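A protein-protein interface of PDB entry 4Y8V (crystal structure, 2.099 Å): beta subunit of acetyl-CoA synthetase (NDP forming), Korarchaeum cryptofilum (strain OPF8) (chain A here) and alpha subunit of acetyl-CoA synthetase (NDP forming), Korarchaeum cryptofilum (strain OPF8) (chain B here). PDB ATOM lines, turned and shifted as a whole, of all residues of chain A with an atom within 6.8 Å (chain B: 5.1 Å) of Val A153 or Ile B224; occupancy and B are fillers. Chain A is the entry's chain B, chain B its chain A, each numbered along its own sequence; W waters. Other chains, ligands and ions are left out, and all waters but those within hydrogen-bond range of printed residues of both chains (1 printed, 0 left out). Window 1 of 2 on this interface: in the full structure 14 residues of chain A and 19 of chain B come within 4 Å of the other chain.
The backbone carbonyl oxygen of Ala A154 lies within hydrogen-bond range of the guanidinium group of Arg B221 (2.8 Å). OE1 of Gln B271 is in hydrogen-bond range of N of Val A153 (2.8 Å).
Water W1 lies within hydrogen-bond range of OD2 of Asp A160 and NE2 of Gln B271.
Among the printed residues, pairs that only touch across the chains: Phe A130 with Ala B268 (3.3 Å), Phe A130 with Gly B220 (3.4 Å), Arg A152 with Gln B271 (3.5 Å), Asp A127 with Ile B264 (3.6 Å), Pro A155 with Arg B221 (3.6 Å), Asp A160 with Gln B271 (3.6 Å), Phe A130 with Ile B264 (3.7 Å), Phe A130 with Ile B224 (3.9 Å), Val A153 with Ile B224 (3.9 Å) and Phe A151 with Ile B264 (3.99 Å).
Of the 14 printed residues of chain A, 8 touch a printed residue of chain B. Hydrophobic or aromatic side chains of chain A within 4 Å of the printed part of chain B: Phe A130, Phe A151, Val A153 and Pro A155. Hydrophobic or aromatic side chains of chain B within 4 Å of the printed part of chain A: Ile B224, Ile B264 and Ala B268. Among the printed residues, no Asp or Glu carboxylate lies within 4 Å of a Lys or Arg side-chain nitrogen of the other chain.
The guanidinium group of Arg B221 lies within salt-bridge range of the side-chain carboxylate of Asp B225, at 2.7 Å. The backbone carbonyl oxygen (O) of Ile B224 lies within hydrogen-bond range of the side-chain hydroxyl (OG) of Ser B228. The side-chain carboxylate of Asp A127 is in hydrogen-bond range of the backbone NH of Phe A130, 3.0 Å away. The backbone NH of Ala A154 sits at hydrogen-bond distance from the backbone carbonyl oxygen of Pro A132 (2.9 Å). The backbone carbonyl oxygen (O) of Arg A152 lies within hydrogen-bond range of the backbone NH (N) of Val A134. The backbone NH (N) of Ser A157 lies within hydrogen-bond range of the side-chain carboxylate (OD2) of Asp A160, at 2.9 Å.
Of the printed residues of chain B, Phe A130 touches Gly B220 (3.4 Å), Ile B224 (3.9 Å), Ile B264 (3.7 Å) and Ala B268 (3.3 Å). Printed residues of chain B within 4 Å of Val A153: Ile B224 (3.9 Å) and Gln B271 (2.8 Å). Of the printed residues of chain B, Asp A160 touches Gln B271 (3.6 Å). Ile B224 touches just these residues of chain A: Phe A130 (3.9 Å) and Val A153 (3.9 Å). Of the printed residues of chain A, Ile B264 touches Asp A127, Phe A130 and Phe A151. The nearest printed residue of chain B that does not touch Val A153 is Arg B221 (4.01 Å).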
ATOM      1  N   ASP A 127     -33.038   1.432 -31.407  1.00  0.00           N
ATOM      2  CA  ASP A 127     -32.650   1.323 -32.799  1.00  0.00           C
ATOM      3  C   ASP A 127     -32.616  -0.157 -33.182  1.00  0.00           C
ATOM      4  O   ASP A 127     -32.152  -0.982 -32.392  1.00  0.00           O
ATOM      5  CB  ASP A 127     -31.288   1.980 -33.027  1.00  0.00           C
ATOM      6  CG  ASP A 127     -30.842   1.909 -34.475  1.00  0.00           C
ATOM      7  OD1 ASP A 127     -31.234   2.795 -35.263  1.00  0.00           O
ATOM      8  OD2 ASP A 127     -30.097   0.968 -34.819  1.00  0.00           O
ATOM      9  N   PHE A 130     -28.784  -1.138 -33.125  1.00  0.00           N
ATOM     10  CA  PHE A 130     -27.918  -0.873 -31.978  1.00  0.00           C
ATOM     11  C   PHE A 130     -28.637  -0.872 -30.624  1.00  0.00           C
ATOM     12  O   PHE A 130     -28.011  -0.646 -29.587  1.00  0.00           O
ATOM     13  CB  PHE A 130     -27.204   0.461 -32.198  1.00  0.00           C
ATOM     14  CG  PHE A 130     -26.334   0.474 -33.423  1.00  0.00           C
ATOM     15  CD1 PHE A 130     -25.101  -0.154 -33.421  1.00  0.00           C
ATOM     16  CD2 PHE A 130     -26.758   1.095 -34.585  1.00  0.00           C
ATOM     17  CE1 PHE A 130     -24.306  -0.154 -34.550  1.00  0.00           C
ATOM     18  CE2 PHE A 130     -25.966   1.099 -35.718  1.00  0.00           C
ATOM     19  CZ  PHE A 130     -24.741   0.475 -35.700  1.00  0.00           C
ATOM     20  N   GLY A 131     -29.943  -1.122 -30.627  1.00  0.00           N
ATOM     21  CA  GLY A 131     -30.685  -1.241 -29.382  1.00  0.00           C
ATOM     22  C   GLY A 131     -30.831   0.095 -28.672  1.00  0.00           C
ATOM     23  O   GLY A 131     -30.844   1.139 -29.326  1.00  0.00           O
ATOM     24  N   PRO A 132     -30.894   0.082 -27.325  1.00  0.00           N
ATOM     25  CA  PRO A 132     -31.159   1.332 -26.599  1.00  0.00           C
ATOM     26  C   PRO A 132     -30.143   2.431 -26.904  1.00  0.00           C
ATOM     27  O   PRO A 132     -28.934   2.234 -26.774  1.00  0.00           O
ATOM     28  CB  PRO A 132     -31.089   0.911 -25.126  1.00  0.00           C
ATOM     29  CG  PRO A 132     -30.314  -0.353 -25.114  1.00  0.00           C
ATOM     30  CD  PRO A 132     -30.626  -1.037 -26.405  1.00  0.00           C
ATOM     31  N   THR A 133     -30.664   3.588 -27.302  1.00  0.00           N
ATOM     32  CA  THR A 133     -29.859   4.718 -27.747  1.00  0.00           C
ATOM     33  C   THR A 133     -30.352   5.990 -27.074  1.00  0.00           C
ATOM     34  O   THR A 133     -31.549   6.285 -27.095  1.00  0.00           O
ATOM     35  CB  THR A 133     -29.925   4.885 -29.280  1.00  0.00           C
ATOM     36  OG1 THR A 133     -29.444   3.694 -29.921  1.00  0.00           O
ATOM     37  CG2 THR A 133     -29.093   6.081 -29.736  1.00  0.00           C
ATOM     38  N   VAL A 134     -29.427   6.744 -26.486  1.00  0.00           N
ATOM     39  CA  VAL A 134     -29.773   7.987 -25.799  1.00  0.00           C
ATOM     40  C   VAL A 134     -29.664   9.169 -26.757  1.00  0.00           C
ATOM     41  O   VAL A 134     -28.741   9.232 -27.572  1.00  0.00           O
ATOM     42  CB  VAL A 134     -28.862   8.230 -24.574  1.00  0.00           C
ATOM     43  CG1 VAL A 134     -29.178   9.575 -23.918  1.00  0.00           C
ATOM     44  CG2 VAL A 134     -29.015   7.101 -23.565  1.00  0.00           C
ATOM     45  N   PHE A 151     -26.656  11.580 -30.584  1.00  0.00           N
ATOM     46  CA  PHE A 151     -27.002  10.218 -30.184  1.00  0.00           C
ATOM     47  C   PHE A 151     -25.782   9.471 -29.671  1.00  0.00           C
ATOM     48  O   PHE A 151     -24.675   9.658 -30.184  1.00  0.00           O
ATOM     49  CB  PHE A 151     -27.594   9.426 -31.353  1.00  0.00           C
ATOM     50  CG  PHE A 151     -28.818  10.043 -31.962  1.00  0.00           C
ATOM     51  CD1 PHE A 151     -28.702  10.998 -32.958  1.00  0.00           C
ATOM     52  CD2 PHE A 151     -30.084   9.643 -31.562  1.00  0.00           C
ATOM     53  CE1 PHE A 151     -29.827  11.562 -33.531  1.00  0.00           C
ATOM     54  CE2 PHE A 151     -31.216  10.201 -32.132  1.00  0.00           C
ATOM     55  CZ  PHE A 151     -31.088  11.161 -33.118  1.00  0.00           C
ATOM     56  N   ARG A 152     -25.990   8.645 -28.648  1.00  0.00           N
ATOM     57  CA  ARG A 152     -25.001   7.651 -28.234  1.00  0.00           C
ATOM     58  C   ARG A 152     -25.696   6.337 -27.890  1.00  0.00           C
ATOM     59  O   ARG A 152     -26.745   6.330 -27.244  1.00  0.00           O
ATOM     60  CB  ARG A 152     -24.188   8.140 -27.034  1.00  0.00           C
ATOM     61  CG  ARG A 152     -23.274   9.322 -27.316  1.00  0.00           C
ATOM     62  CD  ARG A 152     -22.125   8.954 -28.247  1.00  0.00           C
ATOM     63  NE  ARG A 152     -21.161  10.045 -28.358  1.00  0.00           N
ATOM     64  CZ  ARG A 152     -21.333  11.130 -29.108  1.00  0.00           C
ATOM     65  NH1 ARG A 152     -22.438  11.283 -29.825  1.00  0.00           N
ATOM     66  NH2 ARG A 152     -20.398  12.068 -29.136  1.00  0.00           N
ATOM     67  N   VAL A 153     -25.106   5.229 -28.322  1.00  0.00           N
ATOM     68  CA  VAL A 153     -25.652   3.908 -28.045  1.00  0.00           C
ATOM     69  C   VAL A 153     -25.296   3.517 -26.616  1.00  0.00           C
ATOM     70  O   VAL A 153     -24.159   3.701 -26.180  1.00  0.00           O
ATOM     71  CB  VAL A 153     -25.120   2.851 -29.037  1.00  0.00           C
ATOM     72  CG1 VAL A 153     -25.755   1.489 -28.768  1.00  0.00           C
ATOM     73  CG2 VAL A 153     -25.393   3.286 -30.471  1.00  0.00           C
ATOM     74  N   ALA A 154     -26.272   2.981 -25.890  1.00  0.00           N
ATOM     75  CA  ALA A 154     -26.090   2.673 -24.477  1.00  0.00           C
ATOM     76  C   ALA A 154     -25.441   1.304 -24.298  1.00  0.00           C
ATOM     77  O   ALA A 154     -25.563   0.444 -25.171  1.00  0.00           O
ATOM     78  CB  ALA A 154     -27.427   2.729 -23.751  1.00  0.00           C
ATOM     79  N   PRO A 155     -24.747   1.090 -23.165  1.00  0.00           N
ATOM     80  CA  PRO A 155     -24.548   2.042 -22.064  1.00  0.00           C
ATOM     81  C   PRO A 155     -23.577   3.174 -22.397  1.00  0.00           C
ATOM     82  O   PRO A 155     -22.659   2.991 -23.199  1.00  0.00           O
ATOM     83  CB  PRO A 155     -23.989   1.161 -20.944  1.00  0.00           C
ATOM     84  CG  PRO A 155     -23.290   0.062 -21.654  1.00  0.00           C
ATOM     85  CD  PRO A 155     -24.120  -0.213 -22.877  1.00  0.00           C
ATOM     86  N   LEU A 156     -23.792   4.329 -21.773  1.00  0.00           N
ATOM     87  CA  LEU A 156     -22.962   5.507 -21.994  1.00  0.00           C
ATOM     88  C   LEU A 156     -21.839   5.614 -20.968  1.00  0.00           C
ATOM     89  O   LEU A 156     -22.077   5.533 -19.764  1.00  0.00           O
ATOM     90  CB  LEU A 156     -23.812   6.778 -21.932  1.00  0.00           C
ATOM     91  CG  LEU A 156     -24.511   7.258 -23.205  1.00  0.00           C
ATOM     92  CD1 LEU A 156     -25.425   6.190 -23.775  1.00  0.00           C
ATOM     93  CD2 LEU A 156     -25.290   8.531 -22.908  1.00  0.00           C
ATOM     94  N   SER A 157     -20.617   5.794 -21.456  1.00  0.00           N
ATOM     95  CA  SER A 157     -19.493   6.173 -20.605  1.00  0.00           C
ATOM     96  C   SER A 157     -19.560   7.678 -20.356  1.00  0.00           C
ATOM     97  O   SER A 157     -20.319   8.385 -21.023  1.00  0.00           O
ATOM     98  CB  SER A 157     -18.166   5.810 -21.263  1.00  0.00           C
ATOM     99  OG  SER A 157     -17.961   6.653 -22.380  1.00  0.00           O
ATOM    100  N   ASP A 160     -18.783   9.303 -23.523  1.00  0.00           N
ATOM    101  CA  ASP A 160     -19.927   9.384 -24.426  1.00  0.00           C
ATOM    102  C   ASP A 160     -20.829  10.562 -24.062  1.00  0.00           C
ATOM    103  O   ASP A 160     -21.212  11.360 -24.924  1.00  0.00           O
ATOM    104  CB  ASP A 160     -20.732   8.082 -24.391  1.00  0.00           C
ATOM    105  CG  ASP A 160     -19.955   6.898 -24.935  1.00  0.00           C
ATOM    106  OD1 ASP A 160     -19.295   7.051 -25.983  1.00  0.00           O
ATOM    107  OD2 ASP A 160     -19.998   5.814 -24.309  1.00  0.00           O
ATOM    108  N   GLY B 220     -25.869  -4.768 -33.712  1.00  0.00           N
ATOM    109  CA  GLY B 220     -25.111  -3.543 -33.517  1.00  0.00           C
ATOM    110  C   GLY B 220     -24.317  -3.423 -32.232  1.00  0.00           C
ATOM    111  O   GLY B 220     -23.182  -2.944 -32.251  1.00  0.00           O
ATOM    112  N   ARG B 221     -24.906  -3.839 -31.117  1.00  0.00           N
ATOM    113  CA  ARG B 221     -24.236  -3.732 -29.826  1.00  0.00           C
ATOM    114  C   ARG B 221     -22.930  -4.520 -29.843  1.00  0.00           C
ATOM    115  O   ARG B 221     -21.871  -4.032 -29.435  1.00  0.00           O
ATOM    116  CB  ARG B 221     -25.148  -4.239 -28.707  1.00  0.00           C
ATOM    117  CG  ARG B 221     -24.542  -4.153 -27.318  1.00  0.00           C
ATOM    118  CD  ARG B 221     -24.249  -2.711 -26.937  1.00  0.00           C
ATOM    119  NE  ARG B 221     -22.823  -2.409 -27.005  1.00  0.00           N
ATOM    120  CZ  ARG B 221     -22.290  -1.227 -26.714  1.00  0.00           C
ATOM    121  NH1 ARG B 221     -23.063  -0.220 -26.330  1.00  0.00           N
ATOM    122  NH2 ARG B 221     -20.979  -1.052 -26.808  1.00  0.00           N
ATOM    123  N   MET B 222     -23.027  -5.746 -30.334  1.00  0.00           N
ATOM    124  CA  MET B 222     -21.884  -6.632 -30.465  1.00  0.00           C
ATOM    125  C   MET B 222     -20.863  -6.050 -31.449  1.00  0.00           C
ATOM    126  O   MET B 222     -19.653  -6.162 -31.238  1.00  0.00           O
ATOM    127  CB  MET B 222     -22.368  -8.019 -30.910  1.00  0.00           C
ATOM    128  CG  MET B 222     -21.288  -9.080 -31.064  1.00  0.00           C
ATOM    129  SD  MET B 222     -20.390  -9.546 -29.566  1.00  0.00           S
ATOM    130  CE  MET B 222     -21.615  -9.335 -28.278  1.00  0.00           C
ATOM    131  N   PHE B 223     -21.352  -5.424 -32.517  1.00  0.00           N
ATOM    132  CA  PHE B 223     -20.469  -4.776 -33.486  1.00  0.00           C
ATOM    133  C   PHE B 223     -19.590  -3.731 -32.804  1.00  0.00           C
ATOM    134  O   PHE B 223     -18.381  -3.678 -33.039  1.00  0.00           O
ATOM    135  CB  PHE B 223     -21.276  -4.130 -34.617  1.00  0.00           C
ATOM    136  CG  PHE B 223     -20.427  -3.480 -35.679  1.00  0.00           C
ATOM    137  CD1 PHE B 223     -19.979  -2.177 -35.529  1.00  0.00           C
ATOM    138  CD2 PHE B 223     -20.083  -4.174 -36.828  1.00  0.00           C
ATOM    139  CE1 PHE B 223     -19.200  -1.580 -36.503  1.00  0.00           C
ATOM    140  CE2 PHE B 223     -19.303  -3.582 -37.806  1.00  0.00           C
ATOM    141  CZ  PHE B 223     -18.862  -2.282 -37.644  1.00  0.00           C
ATOM    142  N   ILE B 224     -20.197  -2.904 -31.957  1.00  0.00           N
ATOM    143  CA  ILE B 224     -19.453  -1.880 -31.232  1.00  0.00           C
ATOM    144  C   ILE B 224     -18.465  -2.493 -30.243  1.00  0.00           C
ATOM    145  O   ILE B 224     -17.326  -2.039 -30.137  1.00  0.00           O
ATOM    146  CB  ILE B 224     -20.399  -0.920 -30.468  1.00  0.00           C
ATOM    147  CG1 ILE B 224     -21.259  -0.128 -31.454  1.00  0.00           C
ATOM    148  CG2 ILE B 224     -19.599   0.046 -29.580  1.00  0.00           C
ATOM    149  CD1 ILE B 224     -22.378   0.668 -30.802  1.00  0.00           C
ATOM    150  N   ASP B 225     -18.902  -3.503 -29.493  1.00  0.00           N
ATOM    151  CA  ASP B 225     -18.035  -4.133 -28.497  1.00  0.00           C
ATOM    152  C   ASP B 225     -16.761  -4.677 -29.141  1.00  0.00           C
ATOM    153  O   ASP B 225     -15.655  -4.502 -28.623  1.00  0.00           O
ATOM    154  CB  ASP B 225     -18.775  -5.263 -27.773  1.00  0.00           C
ATOM    155  CG  ASP B 225     -19.881  -4.756 -26.857  1.00  0.00           C
ATOM    156  OD1 ASP B 225     -19.887  -3.552 -26.522  1.00  0.00           O
ATOM    157  OD2 ASP B 225     -20.744  -5.572 -26.466  1.00  0.00           O
ATOM    158  N   VAL B 226     -16.922  -5.327 -30.288  1.00  0.00           N
ATOM    159  CA  VAL B 226     -15.803  -5.984 -30.950  1.00  0.00           C
ATOM    160  C   VAL B 226     -14.930  -4.973 -31.693  1.00  0.00           C
ATOM    161  O   VAL B 226     -13.702  -5.021 -31.607  1.00  0.00           O
ATOM    162  CB  VAL B 226     -16.306  -7.064 -31.926  1.00  0.00           C
ATOM    163  CG1 VAL B 226     -15.146  -7.707 -32.683  1.00  0.00           C
ATOM    164  CG2 VAL B 226     -17.091  -8.126 -31.166  1.00  0.00           C
ATOM    165  N   ALA B 227     -15.564  -4.055 -32.414  1.00  0.00           N
ATOM    166  CA  ALA B 227     -14.835  -3.069 -33.205  1.00  0.00           C
ATOM    167  C   ALA B 227     -14.024  -2.107 -32.342  1.00  0.00           C
ATOM    168  O   ALA B 227     -12.949  -1.663 -32.746  1.00  0.00           O
ATOM    169  CB  ALA B 227     -15.793  -2.290 -34.088  1.00  0.00           C
ATOM    170  N   SER B 228     -14.554  -1.734 -31.180  1.00  0.00           N
ATOM    171  CA  SER B 228     -13.846  -0.787 -30.324  1.00  0.00           C
ATOM    172  C   SER B 228     -12.576  -1.438 -29.780  1.00  0.00           C
ATOM    173  O   SER B 228     -11.517  -0.805 -29.732  1.00  0.00           O
ATOM    174  CB  SER B 228     -14.742  -0.290 -29.185  1.00  0.00           C
ATOM    175  OG  SER B 228     -15.200  -1.356 -28.379  1.00  0.00           O
ATOM    176  N   ARG B 229     -12.663  -2.716 -29.420  1.00  0.00           N
ATOM    177  CA  ARG B 229     -11.490  -3.412 -28.902  1.00  0.00           C
ATOM    178  C   ARG B 229     -10.444  -3.573 -30.006  1.00  0.00           C
ATOM    179  O   ARG B 229      -9.258  -3.336 -29.772  1.00  0.00           O
ATOM    180  CB  ARG B 229     -11.874  -4.770 -28.282  1.00  0.00           C
ATOM    181  CG  ARG B 229     -12.003  -5.988 -29.213  1.00  0.00           C
ATOM    182  CD  ARG B 229     -11.630  -7.264 -28.467  1.00  0.00           C
ATOM    183  NE  ARG B 229     -12.422  -8.421 -28.880  1.00  0.00           N
ATOM    184  CZ  ARG B 229     -13.628  -8.717 -28.400  1.00  0.00           C
ATOM    185  NH1 ARG B 229     -14.199  -7.934 -27.491  1.00  0.00           N
ATOM    186  NH2 ARG B 229     -14.268  -9.794 -28.831  1.00  0.00           N
ATOM    187  N   ILE B 264     -27.338   7.501 -36.113  1.00  0.00           N
ATOM    188  CA  ILE B 264     -26.994   6.521 -35.092  1.00  0.00           C
ATOM    189  C   ILE B 264     -25.852   5.621 -35.563  1.00  0.00           C
ATOM    190  O   ILE B 264     -25.000   5.240 -34.759  1.00  0.00           O
ATOM    191  CB  ILE B 264     -28.222   5.686 -34.685  1.00  0.00           C
ATOM    192  CG1 ILE B 264     -29.245   6.593 -33.990  1.00  0.00           C
ATOM    193  CG2 ILE B 264     -27.821   4.548 -33.745  1.00  0.00           C
ATOM    194  CD1 ILE B 264     -30.590   5.944 -33.716  1.00  0.00           C
ATOM    195  N   ALA B 268     -22.372   5.109 -33.627  1.00  0.00           N
ATOM    196  CA  ALA B 268     -21.831   3.775 -33.394  1.00  0.00           C
ATOM    197  C   ALA B 268     -20.387   3.666 -33.882  1.00  0.00           C
ATOM    198  O   ALA B 268     -19.551   3.039 -33.236  1.00  0.00           O
ATOM    199  CB  ALA B 268     -22.696   2.725 -34.066  1.00  0.00           C
ATOM    200  N   GLN B 271     -18.157   5.548 -31.479  1.00  0.00           N
ATOM    201  CA  GLN B 271     -17.955   4.780 -30.252  1.00  0.00           C
ATOM    202  C   GLN B 271     -17.081   3.554 -30.527  1.00  0.00           C
ATOM    203  O   GLN B 271     -16.474   2.987 -29.619  1.00  0.00           O
ATOM    204  CB  GLN B 271     -19.301   4.369 -29.647  1.00  0.00           C
ATOM    205  CG  GLN B 271     -20.131   5.553 -29.165  1.00  0.00           C
ATOM    206  CD  GLN B 271     -21.533   5.165 -28.733  1.00  0.00           C
ATOM    207  OE1 GLN B 271     -22.505   5.466 -29.422  1.00  0.00           O
ATOM    208  NE2 GLN B 271     -21.645   4.512 -27.582  1.00  0.00           N
ATOM    209  N   SER B 272     -16.991   3.160 -31.793  1.00  0.00           N
ATOM    210  CA  SER B 272     -16.148   2.030 -32.188  1.00  0.00           C
ATOM    211  C   SER B 272     -14.718   2.445 -32.539  1.00  0.00           C
ATOM    212  O   SER B 272     -13.856   1.591 -32.744  1.00  0.00           O
ATOM    213  CB  SER B 272     -16.770   1.299 -33.376  1.00  0.00           C
ATOM    214  OG  SER B 272     -17.984   0.676 -33.001  1.00  0.00           O
HETATM  215  O   HOH W   1     -19.270   3.822 -25.985  1.00  0.00           O
